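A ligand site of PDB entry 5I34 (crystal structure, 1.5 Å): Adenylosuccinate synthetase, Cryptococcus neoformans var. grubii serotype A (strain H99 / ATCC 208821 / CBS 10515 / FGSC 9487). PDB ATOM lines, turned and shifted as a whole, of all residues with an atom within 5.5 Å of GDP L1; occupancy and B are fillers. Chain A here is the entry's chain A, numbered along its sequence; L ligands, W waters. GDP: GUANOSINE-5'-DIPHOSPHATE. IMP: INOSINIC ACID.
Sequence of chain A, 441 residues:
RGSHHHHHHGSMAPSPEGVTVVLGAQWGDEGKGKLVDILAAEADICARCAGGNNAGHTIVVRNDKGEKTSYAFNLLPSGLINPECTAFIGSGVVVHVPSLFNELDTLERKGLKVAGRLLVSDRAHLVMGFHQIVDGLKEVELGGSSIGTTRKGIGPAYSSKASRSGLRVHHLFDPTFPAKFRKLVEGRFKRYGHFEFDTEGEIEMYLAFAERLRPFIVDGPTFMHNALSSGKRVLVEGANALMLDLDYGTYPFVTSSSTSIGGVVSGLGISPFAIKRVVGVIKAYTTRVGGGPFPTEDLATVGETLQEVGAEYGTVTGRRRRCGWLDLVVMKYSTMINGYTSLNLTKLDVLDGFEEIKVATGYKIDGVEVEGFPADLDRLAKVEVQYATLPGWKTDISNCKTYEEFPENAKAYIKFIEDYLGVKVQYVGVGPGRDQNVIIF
N of Gly 431 sits at hydrogen-bond distance from O6 of GDP L1, 3.2 Å away. NE2 of His 57 sits at hydrogen-bond distance from O1B of GDP L1. The backbone NH (N) of Val 430 sits at hydrogen-bond distance from an oxygen (O6) of GDP L1, 3.4 Å away. The backbone NH (N) of Lys 32 is in hydrogen-bond range of an oxygen (O3B) of GDP L1, at 2.9 Å. The side-chain carboxylate of Asp 349 is in hydrogen-bond range of a nitrogen (N1) of GDP L1. The side-chain carboxylate (OD2) of Asp 29 is in hydrogen-bond range of a nitrogen (N1) of IMP L2 (3.3 Å). O3B of GDP L1 lies within salt-bridge range of NZ of Lys 32 (2.8 Å). The backbone NH of Gly 31 sits at hydrogen-bond distance from an oxygen (O3B) of GDP L1 (2.9 Å). N of Lys 347 is in hydrogen-bond range of O6 of GDP L1 (3.1 Å). O4' of GDP L1 sits close to NZ of Lys 347. O1A of GDP L1 sits at hydrogen-bond distance from N of Gly 33, 2.8 Å away. O3B of GDP L1 is in hydrogen-bond range of N of Glu 30 (3.4 Å).
An oxygen (O2A) of GDP L1 sits close to the backbone carbonyl oxygen (O) of Gly 56 (3.4 Å). An oxygen (O6) of GDP L1 lies close to the backbone carbonyl oxygen of Gly 429, 3.3 Å away. Asp 29 touches GDP L1 (CA to O2B, 3.5 Å). Lys 34 touches GDP L1. Val 350 touches GDP L1. Pro 432 touches GDP L1 (N to C2, 3.7 Å). Of the 23 residues printed, 15 come within 4 Å of GDP L1. The nearest printed residue that does not touch GDP L1 is Thr 346 (4.2 Å).
The backbone carbonyl oxygen (O) of Gly 429 sits at hydrogen-bond distance from the backbone NH (N) of Leu 348, 3.1 Å away. N of Gly 431 sits at hydrogen-bond distance from OD1 of Asp 349 (3.3 Å). The side-chain amino group (NZ) of Lys 32 lies within salt-bridge range of the side-chain carboxylate (OE1) of Glu 30 (3.1 Å). OE2 of Glu 30 is in hydrogen-bond range of N of Gly 28, 2.9 Å away. O of Glu 30 sits at hydrogen-bond distance from OG1 of Thr 346, at 2.6 Å. The backbone NH (N) of Lys 347 is in hydrogen-bond range of the backbone carbonyl oxygen (O) of Gly 429 (3.4 Å). The backbone carbonyl oxygen (O) of Gly 310 is in hydrogen-bond range of the side-chain amino group (NZ) of Lys 347, at 3.2 Å. O of Gln 436 is in hydrogen-bond range of NZ of Lys 34.
Water W1 lies within hydrogen-bond range of an oxygen (O2B) of GDP L1 (2.9 Å) and the backbone carbonyl oxygen (O) of Gly 56 (3.0 Å). Water W5 lies within hydrogen-bond range of N7 of GDP L1 (2.9 Å) and NZ of Lys 34 (3.1 Å). Water W4 bridges the backbone carbonyl oxygen of Val 309 (2.9 Å) and a nitrogen (N2) of GDP L1 (2.9 Å). Water W2 lies within hydrogen-bond range of the backbone carbonyl oxygen (O) of Pro 432 and an oxygen (O2') of GDP L1. Water W3 lies within hydrogen-bond range of NZ of Lys 347 (2.8 Å) and O of Asp 29 (2.8 Å).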
ATOM      1  N   GLY A  28      -9.566  -3.420 -11.920  1.00  0.00           N
ATOM      2  CA  GLY A  28      -9.385  -4.745 -11.346  1.00  0.00           C
ATOM      3  C   GLY A  28     -10.514  -5.213 -10.450  1.00  0.00           C
ATOM      4  O   GLY A  28     -11.442  -4.457 -10.139  1.00  0.00           O
ATOM      5  N   ASP A  29     -10.426  -6.488 -10.061  1.00  0.00           N
ATOM      6  CA  ASP A  29     -11.422  -7.075  -9.169  1.00  0.00           C
ATOM      7  C   ASP A  29     -12.819  -7.038  -9.768  1.00  0.00           C
ATOM      8  O   ASP A  29     -13.812  -7.033  -9.038  1.00  0.00           O
ATOM      9  CB  ASP A  29     -11.402  -6.367  -7.810  1.00  0.00           C
ATOM     10  CG  ASP A  29     -10.002  -6.273  -7.231  1.00  0.00           C
ATOM     11  OD1 ASP A  29      -9.552  -5.161  -6.904  1.00  0.00           O
ATOM     12  OD2 ASP A  29      -9.331  -7.331  -7.132  1.00  0.00           O
ATOM     13  N   GLU A  30     -12.913  -7.016 -11.088  1.00  0.00           N
ATOM     14  CA  GLU A  30     -14.238  -6.946 -11.705  1.00  0.00           C
ATOM     15  C   GLU A  30     -15.005  -8.245 -11.566  1.00  0.00           C
ATOM     16  O   GLU A  30     -16.236  -8.232 -11.488  1.00  0.00           O
ATOM     17  CB  GLU A  30     -14.125  -6.600 -13.189  1.00  0.00           C
ATOM     18  CG  GLU A  30     -13.554  -5.194 -13.455  1.00  0.00           C
ATOM     19  CD  GLU A  30     -12.038  -5.143 -13.540  1.00  0.00           C
ATOM     20  OE1 GLU A  30     -11.336  -6.156 -13.282  1.00  0.00           O
ATOM     21  OE2 GLU A  30     -11.569  -4.041 -13.907  1.00  0.00           O
ATOM     22  N   GLY A  31     -14.283  -9.355 -11.505  1.00  0.00           N
ATOM     23  CA  GLY A  31     -14.905 -10.665 -11.513  1.00  0.00           C
ATOM     24  C   GLY A  31     -14.675 -11.451 -12.805  1.00  0.00           C
ATOM     25  O   GLY A  31     -15.617 -12.048 -13.323  1.00  0.00           O
ATOM     26  N   LYS A  32     -13.431 -11.455 -13.281  1.00  0.00           N
ATOM     27  CA  LYS A  32     -13.053 -12.099 -14.548  1.00  0.00           C
ATOM     28  C   LYS A  32     -13.149 -13.623 -14.507  1.00  0.00           C
ATOM     29  O   LYS A  32     -13.318 -14.264 -15.545  1.00  0.00           O
ATOM     30  CB  LYS A  32     -11.591 -11.736 -14.926  1.00  0.00           C
ATOM     31  CG  LYS A  32     -11.372 -10.253 -15.214  1.00  0.00           C
ATOM     32  CD  LYS A  32      -9.896  -9.882 -15.597  1.00  0.00           C
ATOM     33  CE  LYS A  32      -9.007  -9.659 -14.367  1.00  0.00           C
ATOM     34  NZ  LYS A  32      -9.538  -8.627 -13.397  1.00  0.00           N
ATOM     35  N   GLY A  33     -13.002 -14.194 -13.317  1.00  0.00           N
ATOM     36  CA  GLY A  33     -12.857 -15.628 -13.158  1.00  0.00           C
ATOM     37  C   GLY A  33     -14.003 -16.430 -13.729  1.00  0.00           C
ATOM     38  O   GLY A  33     -13.791 -17.450 -14.385  1.00  0.00           O
ATOM     39  N   LYS A  34     -15.235 -15.993 -13.469  1.00  0.00           N
ATOM     40  CA  LYS A  34     -16.395 -16.736 -13.935  1.00  0.00           C
ATOM     41  C   LYS A  34     -16.426 -16.804 -15.455  1.00  0.00           C
ATOM     42  O   LYS A  34     -16.702 -17.871 -16.024  1.00  0.00           O
ATOM     43  CB  LYS A  34     -17.674 -16.108 -13.379  1.00  0.00           C
ATOM     44  CG  LYS A  34     -17.947 -16.547 -11.937  1.00  0.00           C
ATOM     45  CD  LYS A  34     -19.013 -15.723 -11.269  1.00  0.00           C
ATOM     46  CE  LYS A  34     -20.353 -16.059 -11.825  1.00  0.00           C
ATOM     47  NZ  LYS A  34     -21.259 -14.921 -11.788  1.00  0.00           N
ATOM     48  N   ALA A  55      -3.606 -12.834 -10.296  1.00  0.00           N
ATOM     49  CA  ALA A  55      -4.770 -13.285 -11.063  1.00  0.00           C
ATOM     50  C   ALA A  55      -5.449 -14.419 -10.312  1.00  0.00           C
ATOM     51  O   ALA A  55      -5.886 -15.398 -10.908  1.00  0.00           O
ATOM     52  CB  ALA A  55      -4.352 -13.731 -12.462  1.00  0.00           C
ATOM     53  N   GLY A  56      -5.524 -14.260  -8.989  1.00  0.00           N
ATOM     54  CA  GLY A  56      -6.111 -15.250  -8.124  1.00  0.00           C
ATOM     55  C   GLY A  56      -7.574 -15.529  -8.428  1.00  0.00           C
ATOM     56  O   GLY A  56      -8.407 -14.633  -8.350  1.00  0.00           O
ATOM     57  N   HIS A  57      -7.873 -16.776  -8.800  1.00  0.00           N
ATOM     58  CA  HIS A  57      -9.240 -17.250  -8.991  1.00  0.00           C
ATOM     59  C   HIS A  57      -9.476 -18.515  -8.218  1.00  0.00           C
ATOM     60  O   HIS A  57      -8.590 -19.345  -8.123  1.00  0.00           O
ATOM     61  CB  HIS A  57      -9.517 -17.554 -10.469  1.00  0.00           C
ATOM     62  CG  HIS A  57      -9.510 -16.346 -11.328  1.00  0.00           C
ATOM     63  ND1 HIS A  57      -9.025 -16.346 -12.615  1.00  0.00           N
ATOM     64  CD2 HIS A  57      -9.925 -15.082 -11.081  1.00  0.00           C
ATOM     65  CE1 HIS A  57      -9.140 -15.129 -13.129  1.00  0.00           C
ATOM     66  NE2 HIS A  57      -9.684 -14.349 -12.212  1.00  0.00           N
ATOM     67  N   THR A  58     -10.676 -18.671  -7.691  1.00  0.00           N
ATOM     68  CA  THR A  58     -11.112 -19.965  -7.210  1.00  0.00           C
ATOM     69  C   THR A  58     -12.301 -20.382  -8.019  1.00  0.00           C
ATOM     70  O   THR A  58     -13.245 -19.610  -8.189  1.00  0.00           O
ATOM     71  CB  THR A  58     -11.476 -19.933  -5.724  1.00  0.00           C
ATOM     72  OG1 THR A  58     -10.299 -19.638  -4.954  1.00  0.00           O
ATOM     73  CG2 THR A  58     -12.030 -21.278  -5.276  1.00  0.00           C
ATOM     74  N   VAL A 309     -21.940  -5.503   0.554  1.00  0.00           N
ATOM     75  CA  VAL A 309     -22.729  -6.418  -0.261  1.00  0.00           C
ATOM     76  C   VAL A 309     -21.854  -7.063  -1.343  1.00  0.00           C
ATOM     77  O   VAL A 309     -22.022  -8.235  -1.647  1.00  0.00           O
ATOM     78  CB  VAL A 309     -23.941  -5.707  -0.885  1.00  0.00           C
ATOM     79  CG1 VAL A 309     -24.753  -6.636  -1.794  1.00  0.00           C
ATOM     80  CG2 VAL A 309     -24.846  -5.144   0.200  1.00  0.00           C
ATOM     81  N   GLY A 310     -20.921  -6.302  -1.911  1.00  0.00           N
ATOM     82  CA  GLY A 310     -19.994  -6.836  -2.895  1.00  0.00           C
ATOM     83  C   GLY A 310     -18.816  -7.590  -2.303  1.00  0.00           C
ATOM     84  O   GLY A 310     -17.953  -8.066  -3.065  1.00  0.00           O
ATOM     85  N   THR A 346     -20.687  -7.613 -14.508  1.00  0.00           N
ATOM     86  CA  THR A 346     -20.584  -8.444 -13.332  1.00  0.00           C
ATOM     87  C   THR A 346     -21.146  -7.781 -12.071  1.00  0.00           C
ATOM     88  O   THR A 346     -21.241  -6.558 -11.947  1.00  0.00           O
ATOM     89  CB  THR A 346     -19.119  -8.806 -13.048  1.00  0.00           C
ATOM     90  OG1 THR A 346     -18.391  -7.580 -12.832  1.00  0.00           O
ATOM     91  CG2 THR A 346     -18.521  -9.585 -14.228  1.00  0.00           C
ATOM     92  N   LYS A 347     -21.476  -8.633 -11.105  1.00  0.00           N
ATOM     93  CA  LYS A 347     -21.986  -8.225  -9.806  1.00  0.00           C
ATOM     94  C   LYS A 347     -23.196  -7.342  -9.922  1.00  0.00           C
ATOM     95  O   LYS A 347     -23.414  -6.460  -9.096  1.00  0.00           O
ATOM     96  CB  LYS A 347     -20.880  -7.538  -8.997  1.00  0.00           C
ATOM     97  CG  LYS A 347     -19.614  -8.340  -8.864  1.00  0.00           C
ATOM     98  CD  LYS A 347     -18.947  -8.110  -7.499  1.00  0.00           C
ATOM     99  CE  LYS A 347     -17.538  -8.613  -7.447  1.00  0.00           C
ATOM    100  NZ  LYS A 347     -16.936  -8.461  -6.077  1.00  0.00           N
ATOM    101  N   LEU A 348     -24.038  -7.607 -10.906  1.00  0.00           N
ATOM    102  CA  LEU A 348     -25.246  -6.805 -11.053  1.00  0.00           C
ATOM    103  C   LEU A 348     -26.148  -7.001  -9.823  1.00  0.00           C
ATOM    104  O   LEU A 348     -26.888  -6.096  -9.437  1.00  0.00           O
ATOM    105  CB  LEU A 348     -26.005  -7.166 -12.334  1.00  0.00           C
ATOM    106  CG  LEU A 348     -27.215  -6.279 -12.659  1.00  0.00           C
ATOM    107  CD1 LEU A 348     -26.787  -4.838 -12.795  1.00  0.00           C
ATOM    108  CD2 LEU A 348     -27.953  -6.702 -13.940  1.00  0.00           C
ATOM    109  N   ASP A 349     -26.095  -8.187  -9.214  1.00  0.00           N
ATOM    110  CA  ASP A 349     -26.868  -8.505  -8.012  1.00  0.00           C
ATOM    111  C   ASP A 349     -26.536  -7.607  -6.829  1.00  0.00           C
ATOM    112  O   ASP A 349     -27.342  -7.461  -5.909  1.00  0.00           O
ATOM    113  CB  ASP A 349     -26.640  -9.969  -7.623  1.00  0.00           C
ATOM    114  CG  ASP A 349     -25.172 -10.289  -7.384  1.00  0.00           C
ATOM    115  OD1 ASP A 349     -24.381 -10.176  -8.352  1.00  0.00           O
ATOM    116  OD2 ASP A 349     -24.814 -10.677  -6.245  1.00  0.00           O
ATOM    117  N   VAL A 350     -25.347  -7.009  -6.827  1.00  0.00           N
ATOM    118  CA  VAL A 350     -24.927  -6.176  -5.698  1.00  0.00           C
ATOM    119  C   VAL A 350     -25.783  -4.904  -5.636  1.00  0.00           C
ATOM    120  O   VAL A 350     -25.899  -4.285  -4.583  1.00  0.00           O
ATOM    121  CB  VAL A 350     -23.408  -5.840  -5.788  1.00  0.00           C
ATOM    122  CG1 VAL A 350     -22.984  -4.763  -4.781  1.00  0.00           C
ATOM    123  CG2 VAL A 350     -22.590  -7.113  -5.603  1.00  0.00           C
ATOM    124  N   GLY A 429     -23.212 -11.315 -14.715  1.00  0.00           N
ATOM    125  CA  GLY A 429     -22.958 -11.986 -13.450  1.00  0.00           C
ATOM    126  C   GLY A 429     -24.001 -11.567 -12.448  1.00  0.00           C
ATOM    127  O   GLY A 429     -24.215 -10.361 -12.251  1.00  0.00           O
ATOM    128  N   VAL A 430     -24.663 -12.531 -11.820  1.00  0.00           N
ATOM    129  CA  VAL A 430     -25.713 -12.229 -10.832  1.00  0.00           C
ATOM    130  C   VAL A 430     -25.451 -12.903  -9.480  1.00  0.00           C
ATOM    131  O   VAL A 430     -26.327 -12.952  -8.604  1.00  0.00           O
ATOM    132  CB  VAL A 430     -27.111 -12.646 -11.389  1.00  0.00           C
ATOM    133  CG1 VAL A 430     -27.464 -11.835 -12.634  1.00  0.00           C
ATOM    134  CG2 VAL A 430     -27.190 -14.125 -11.693  1.00  0.00           C
ATOM    135  N   GLY A 431     -24.236 -13.391  -9.280  1.00  0.00           N
ATOM    136  CA  GLY A 431     -23.875 -14.018  -8.030  1.00  0.00           C
ATOM    137  C   GLY A 431     -22.486 -14.617  -8.103  1.00  0.00           C
ATOM    138  O   GLY A 431     -21.931 -14.744  -9.197  1.00  0.00           O
ATOM    139  N   PRO A 432     -21.923 -14.978  -6.961  1.00  0.00           N
ATOM    140  CA  PRO A 432     -20.567 -15.542  -6.880  1.00  0.00           C
ATOM    141  C   PRO A 432     -20.468 -16.996  -7.292  1.00  0.00           C
ATOM    142  O   PRO A 432     -19.362 -17.465  -7.574  1.00  0.00           O
ATOM    143  CB  PRO A 432     -20.220 -15.386  -5.400  1.00  0.00           C
ATOM    144  CG  PRO A 432     -21.523 -15.517  -4.716  1.00  0.00           C
ATOM    145  CD  PRO A 432     -22.531 -14.843  -5.628  1.00  0.00           C
ATOM    146  N   GLN A 436     -24.028 -18.739 -11.650  1.00  0.00           N
ATOM    147  CA  GLN A 436     -24.872 -17.556 -11.469  1.00  0.00           C
ATOM    148  C   GLN A 436     -24.519 -16.538 -12.545  1.00  0.00           C
ATOM    149  O   GLN A 436     -23.952 -15.467 -12.286  1.00  0.00           O
ATOM    150  CB  GLN A 436     -24.722 -16.984 -10.068  1.00  0.00           C
ATOM    151  CG  GLN A 436     -25.405 -17.871  -9.023  1.00  0.00           C
ATOM    152  CD  GLN A 436     -25.341 -17.340  -7.600  1.00  0.00           C
ATOM    153  OE1 GLN A 436     -24.292 -17.313  -6.972  1.00  0.00           O
ATOM    154  NE2 GLN A 436     -26.499 -16.929  -7.087  1.00  0.00           N
HETATM  155  PB  GDP L   1     -10.849 -10.874 -10.839  1.00  0.00           P
HETATM  156  O1B GDP L   1     -10.067 -11.955 -11.555  1.00  0.00           O
HETATM  157  O2B GDP L   1      -9.913 -10.110  -9.913  1.00  0.00           O
HETATM  158  O3B GDP L   1     -11.460  -9.976 -11.834  1.00  0.00           O
HETATM  159  O3A GDP L   1     -12.075 -11.413 -10.003  1.00  0.00           O
HETATM  160  PA  GDP L   1     -12.515 -12.797  -9.461  1.00  0.00           P
HETATM  161  O1A GDP L   1     -13.005 -13.733 -10.517  1.00  0.00           O
HETATM  162  O2A GDP L   1     -11.539 -13.366  -8.486  1.00  0.00           O
HETATM  163  O5' GDP L   1     -13.856 -12.363  -8.659  1.00  0.00           O
HETATM  164  C5' GDP L   1     -13.732 -11.461  -7.542  1.00  0.00           C
HETATM  165  C4' GDP L   1     -14.841 -11.826  -6.527  1.00  0.00           C
HETATM  166  O4' GDP L   1     -15.994 -11.454  -7.021  1.00  0.00           O
HETATM  167  C3' GDP L   1     -14.933 -13.353  -6.329  1.00  0.00           C
HETATM  168  O3' GDP L   1     -15.084 -13.650  -5.008  1.00  0.00           O
HETATM  169  C2' GDP L   1     -16.186 -13.765  -7.136  1.00  0.00           C
HETATM  170  O2' GDP L   1     -16.764 -15.007  -6.537  1.00  0.00           O
HETATM  171  C1' GDP L   1     -16.977 -12.715  -7.023  1.00  0.00           C
HETATM  172  N9  GDP L   1     -17.923 -12.545  -8.086  1.00  0.00           N
HETATM  173  C8  GDP L   1     -17.713 -12.733  -9.424  1.00  0.00           C
HETATM  174  N7  GDP L   1     -18.848 -12.468 -10.093  1.00  0.00           N
HETATM  175  C5  GDP L   1     -19.772 -12.088  -9.176  1.00  0.00           C
HETATM  176  C6  GDP L   1     -21.210 -11.668  -9.335  1.00  0.00           C
HETATM  177  O6  GDP L   1     -21.753 -11.636 -10.408  1.00  0.00           O
HETATM  178  N1  GDP L   1     -21.895 -11.337  -8.183  1.00  0.00           N
HETATM  179  C2  GDP L   1     -21.294 -11.382  -6.927  1.00  0.00           C
HETATM  180  N2  GDP L   1     -22.050 -11.009  -5.772  1.00  0.00           N
HETATM  181  N3  GDP L   1     -19.928 -11.761  -6.748  1.00  0.00           N
HETATM  182  C4  GDP L   1     -19.191 -12.129  -7.933  1.00  0.00           C
HETATM  183  P   IMP L   2       1.522  -4.129  -8.550  1.00  0.00           P
HETATM  184  O1P IMP L   2       2.834  -3.443  -8.874  1.00  0.00           O
HETATM  185  O2P IMP L   2       1.700  -5.031  -7.348  1.00  0.00           O
HETATM  186  O3P IMP L   2       0.943  -4.737  -9.807  1.00  0.00           O
HETATM  187  O5' IMP L   2       0.487  -2.983  -8.064  1.00  0.00           O
HETATM  188  C5' IMP L   2       0.420  -1.750  -8.766  1.00  0.00           C
HETATM  189  C4' IMP L   2      -0.916  -1.056  -8.617  1.00  0.00           C
HETATM  190  O4' IMP L   2      -1.910  -1.849  -9.322  1.00  0.00           O
HETATM  191  C3' IMP L   2      -1.465  -0.895  -7.204  1.00  0.00           C
HETATM  192  O3' IMP L   2      -2.328   0.251  -7.169  1.00  0.00           O
HETATM  193  C2' IMP L   2      -2.290  -2.170  -7.034  1.00  0.00           C
HETATM  194  O2' IMP L   2      -3.299  -2.122  -6.060  1.00  0.00           O
HETATM  195  C1' IMP L   2      -2.891  -2.297  -8.421  1.00  0.00           C
HETATM  196  N9  IMP L   2      -3.192  -3.675  -8.790  1.00  0.00           N
HETATM  197  C8  IMP L   2      -2.342  -4.601  -9.324  1.00  0.00           C
HETATM  198  N7  IMP L   2      -3.071  -5.722  -9.509  1.00  0.00           N
HETATM  199  C5  IMP L   2      -4.337  -5.496  -9.099  1.00  0.00           C
HETATM  200  C6  IMP L   2      -5.560  -6.381  -9.064  1.00  0.00           C
HETATM  201  O6  IMP L   2      -5.495  -7.536  -9.466  1.00  0.00           O
HETATM  202  N1  IMP L   2      -6.752  -5.843  -8.561  1.00  0.00           N
HETATM  203  C2  IMP L   2      -6.820  -4.493  -8.085  1.00  0.00           C
HETATM  204  N3  IMP L   2      -5.668  -3.640  -8.120  1.00  0.00           N
HETATM  205  C4  IMP L   2      -4.412  -4.207  -8.642  1.00  0.00           C
HETATM  206  O   HOH W   1      -7.722 -11.907  -9.263  1.00  0.00           O
HETATM  207  O   HOH W   2     -17.013 -16.643  -9.044  1.00  0.00           O
HETATM  208  O   HOH W   3     -14.195  -8.286  -6.539  1.00  0.00           O
HETATM  209  O   HOH W   4     -20.838 -10.370  -3.198  1.00  0.00           O
HETATM  210  O   HOH W   5     -19.485 -12.697 -12.926  1.00  0.00           O
